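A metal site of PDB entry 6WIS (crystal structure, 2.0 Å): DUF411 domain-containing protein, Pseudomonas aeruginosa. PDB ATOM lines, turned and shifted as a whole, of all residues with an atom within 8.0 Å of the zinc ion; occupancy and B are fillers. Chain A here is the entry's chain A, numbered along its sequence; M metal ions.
Within 4 Å of the zinc ion: His 8, His 33 and Glu 35. Along chain A the residues within 4 Å of the zinc ion span positions 8 to 35. The nearest printed residue that does not touch the zinc ion is Val 41 (4.01 Å).
The backbone carbonyl oxygen (O) of His 8 lies within hydrogen-bond range of the backbone NH (N) of Thr 56, 2.7 Å away. The backbone NH of Glu 35 lies within hydrogen-bond range of the backbone carbonyl oxygen of Arg 9 (2.9 Å). OE2 of Glu 35 is in hydrogen-bond range of N of Asp 37. N of Arg 9 lies within hydrogen-bond range of O of His 33 (3.1 Å). N of His 33 is in hydrogen-bond range of O of Val 7, 3.1 Å away.
The zinc ion is bound by a ring nitrogen (ND1) of His 8, at 2.1 Å. The zinc ion is bound by NE2 of His 33. OE1 of Glu 35 binds the zinc ion. The zinc ion has three donor atoms within binding distance.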
ATOM      1  N   ASP A   6      10.504  17.237 -13.667  1.00  0.00           N
ATOM      2  CA  ASP A   6      11.429  17.240 -14.798  1.00  0.00           C
ATOM      3  C   ASP A   6      11.483  18.627 -15.437  1.00  0.00           C
ATOM      4  O   ASP A   6      10.439  19.205 -15.764  1.00  0.00           O
ATOM      5  CB  ASP A   6      11.043  16.201 -15.857  1.00  0.00           C
ATOM      6  CG  ASP A   6      12.156  15.987 -16.902  1.00  0.00           C
ATOM      7  OD1 ASP A   6      13.338  15.790 -16.491  1.00  0.00           O
ATOM      8  OD2 ASP A   6      11.848  16.015 -18.109  1.00  0.00           O
ATOM      9  N   VAL A   7      12.683  19.161 -15.599  1.00  0.00           N
ATOM     10  CA  VAL A   7      12.875  20.556 -16.011  1.00  0.00           C
ATOM     11  C   VAL A   7      13.557  20.611 -17.365  1.00  0.00           C
ATOM     12  O   VAL A   7      14.642  20.033 -17.563  1.00  0.00           O
ATOM     13  CB  VAL A   7      13.670  21.336 -14.956  1.00  0.00           C
ATOM     14  CG1 VAL A   7      13.854  22.804 -15.411  1.00  0.00           C
ATOM     15  CG2 VAL A   7      12.934  21.276 -13.601  1.00  0.00           C
ATOM     16  N   HIS A   8      12.929  21.319 -18.308  1.00  0.00           N
ATOM     17  CA  HIS A   8      13.533  21.678 -19.587  1.00  0.00           C
ATOM     18  C   HIS A   8      13.955  23.139 -19.479  1.00  0.00           C
ATOM     19  O   HIS A   8      13.102  24.006 -19.239  1.00  0.00           O
ATOM     20  CB  HIS A   8      12.548  21.509 -20.757  1.00  0.00           C
ATOM     21  CG  HIS A   8      11.680  20.300 -20.649  1.00  0.00           C
ATOM     22  ND1 HIS A   8      11.824  19.199 -21.474  1.00  0.00           N
ATOM     23  CD2 HIS A   8      10.642  20.014 -19.830  1.00  0.00           C
ATOM     24  CE1 HIS A   8      10.928  18.294 -21.161  1.00  0.00           C
ATOM     25  NE2 HIS A   8      10.194  18.761 -20.164  1.00  0.00           N
ATOM     26  N   ARG A   9      15.253  23.412 -19.627  1.00  0.00           N
ATOM     27  CA  ARG A   9      15.742  24.767 -19.340  1.00  0.00           C
ATOM     28  C   ARG A   9      16.558  25.331 -20.488  1.00  0.00           C
ATOM     29  O   ARG A   9      17.210  24.612 -21.247  1.00  0.00           O
ATOM     30  CB  ARG A   9      16.567  24.786 -18.041  1.00  0.00           C
ATOM     31  CG  ARG A   9      17.781  23.868 -18.034  1.00  0.00           C
ATOM     32  CD  ARG A   9      18.625  24.066 -16.773  1.00  0.00           C
ATOM     33  NE  ARG A   9      19.614  23.012 -16.582  1.00  0.00           N
ATOM     34  CZ  ARG A   9      20.902  23.103 -16.910  1.00  0.00           C
ATOM     35  NH1 ARG A   9      21.399  24.204 -17.462  1.00  0.00           N
ATOM     36  NH2 ARG A   9      21.718  22.080 -16.665  1.00  0.00           N
ATOM     37  N   ASP A  32      16.779  17.117 -15.146  1.00  0.00           N
ATOM     38  CA  ASP A  32      16.764  18.276 -16.037  1.00  0.00           C
ATOM     39  C   ASP A  32      17.728  18.103 -17.197  1.00  0.00           C
ATOM     40  O   ASP A  32      18.694  17.340 -17.135  1.00  0.00           O
ATOM     41  CB  ASP A  32      17.119  19.571 -15.297  1.00  0.00           C
ATOM     42  CG  ASP A  32      18.519  19.560 -14.745  1.00  0.00           C
ATOM     43  OD1 ASP A  32      18.773  18.759 -13.822  1.00  0.00           O
ATOM     44  OD2 ASP A  32      19.372  20.361 -15.239  1.00  0.00           O
ATOM     45  N   HIS A  33      17.496  18.904 -18.231  1.00  0.00           N
ATOM     46  CA  HIS A  33      18.415  18.998 -19.356  1.00  0.00           C
ATOM     47  C   HIS A  33      18.231  20.353 -20.012  1.00  0.00           C
ATOM     48  O   HIS A  33      17.155  20.953 -19.946  1.00  0.00           O
ATOM     49  CB  HIS A  33      18.153  17.911 -20.386  1.00  0.00           C
ATOM     50  CG  HIS A  33      16.725  17.840 -20.771  1.00  0.00           C
ATOM     51  ND1 HIS A  33      15.779  17.241 -19.964  1.00  0.00           N
ATOM     52  CD2 HIS A  33      16.054  18.343 -21.830  1.00  0.00           C
ATOM     53  CE1 HIS A  33      14.588  17.355 -20.533  1.00  0.00           C
ATOM     54  NE2 HIS A  33      14.740  18.021 -21.668  1.00  0.00           N
ATOM     55  N   VAL A  34      19.303  20.797 -20.658  1.00  0.00           N
ATOM     56  CA  VAL A  34      19.259  21.909 -21.583  1.00  0.00           C
ATOM     57  C   VAL A  34      18.413  21.534 -22.803  1.00  0.00           C
ATOM     58  O   VAL A  34      18.595  20.465 -23.400  1.00  0.00           O
ATOM     59  CB  VAL A  34      20.701  22.295 -21.942  1.00  0.00           C
ATOM     60  CG1 VAL A  34      20.750  23.408 -22.944  1.00  0.00           C
ATOM     61  CG2 VAL A  34      21.429  22.682 -20.665  1.00  0.00           C
ATOM     62  N   GLU A  35      17.499  22.431 -23.191  1.00  0.00           N
ATOM     63  CA  GLU A  35      16.447  22.154 -24.173  1.00  0.00           C
ATOM     64  C   GLU A  35      16.888  22.440 -25.600  1.00  0.00           C
ATOM     65  O   GLU A  35      17.407  23.519 -25.880  1.00  0.00           O
ATOM     66  CB  GLU A  35      15.206  23.003 -23.882  1.00  0.00           C
ATOM     67  CG  GLU A  35      14.164  22.865 -25.010  1.00  0.00           C
ATOM     68  CD  GLU A  35      13.682  21.485 -24.993  1.00  0.00           C
ATOM     69  OE1 GLU A  35      13.668  21.071 -23.853  1.00  0.00           O
ATOM     70  OE2 GLU A  35      13.415  20.798 -26.015  1.00  0.00           O
ATOM     71  N   ALA A  36      16.630  21.495 -26.522  1.00  0.00           N
ATOM     72  CA  ALA A  36      16.905  21.738 -27.939  1.00  0.00           C
ATOM     73  C   ALA A  36      15.742  22.410 -28.657  1.00  0.00           C
ATOM     74  O   ALA A  36      15.967  23.183 -29.589  1.00  0.00           O
ATOM     75  CB  ALA A  36      17.236  20.425 -28.655  1.00  0.00           C
ATOM     76  N   ASP A  37      14.464  22.133 -28.261  1.00  0.00           N
ATOM     77  CA  ASP A  37      13.314  22.706 -28.983  1.00  0.00           C
ATOM     78  C   ASP A  37      12.297  23.200 -27.947  1.00  0.00           C
ATOM     79  O   ASP A  37      11.324  22.517 -27.618  1.00  0.00           O
ATOM     80  CB  ASP A  37      12.683  21.691 -29.941  1.00  0.00           C
ATOM     81  CG  ASP A  37      11.905  22.375 -31.084  1.00  0.00           C
ATOM     82  OD1 ASP A  37      11.359  23.500 -30.890  1.00  0.00           O
ATOM     83  OD2 ASP A  37      11.868  21.780 -32.176  1.00  0.00           O
ATOM     84  N   MET A  38      12.532  24.411 -27.468  1.00  0.00           N
ATOM     85  CA  MET A  38      11.742  24.939 -26.374  1.00  0.00           C
ATOM     86  C   MET A  38      10.342  25.378 -26.838  1.00  0.00           C
ATOM     87  O   MET A  38       9.374  25.241 -26.083  1.00  0.00           O
ATOM     88  CB  MET A  38      12.470  26.102 -25.694  1.00  0.00           C
ATOM     89  CG  MET A  38      11.710  26.623 -24.481  1.00  0.00           C
ATOM     90  SD  MET A  38      11.699  25.271 -23.033  1.00  0.00           S
ATOM     91  CE  MET A  38      13.363  25.791 -22.205  1.00  0.00           C
ATOM     92  N   VAL A  41       8.324  22.321 -26.706  1.00  0.00           N
ATOM     93  CA  VAL A  41       8.029  21.899 -25.340  1.00  0.00           C
ATOM     94  C   VAL A  41       6.897  22.746 -24.778  1.00  0.00           C
ATOM     95  O   VAL A  41       5.925  22.224 -24.225  1.00  0.00           O
ATOM     96  CB  VAL A  41       9.288  21.989 -24.452  1.00  0.00           C
ATOM     97  CG1 VAL A  41       8.900  21.786 -22.986  1.00  0.00           C
ATOM     98  CG2 VAL A  41      10.338  20.954 -24.869  1.00  0.00           C
ATOM     99  N   THR A  56      10.895  25.300 -18.269  1.00  0.00           N
ATOM    100  CA  THR A  56       9.566  24.702 -18.136  1.00  0.00           C
ATOM    101  C   THR A  56       9.715  23.391 -17.368  1.00  0.00           C
ATOM    102  O   THR A  56      10.448  22.499 -17.807  1.00  0.00           O
ATOM    103  CB  THR A  56       8.915  24.421 -19.502  1.00  0.00           C
ATOM    104  OG1 THR A  56       8.889  25.630 -20.282  1.00  0.00           O
ATOM    105  CG2 THR A  56       7.479  23.915 -19.295  1.00  0.00           C
HETATM  106 ZN    ZN M   1      13.293  19.021 -22.961  1.00  0.00          ZN
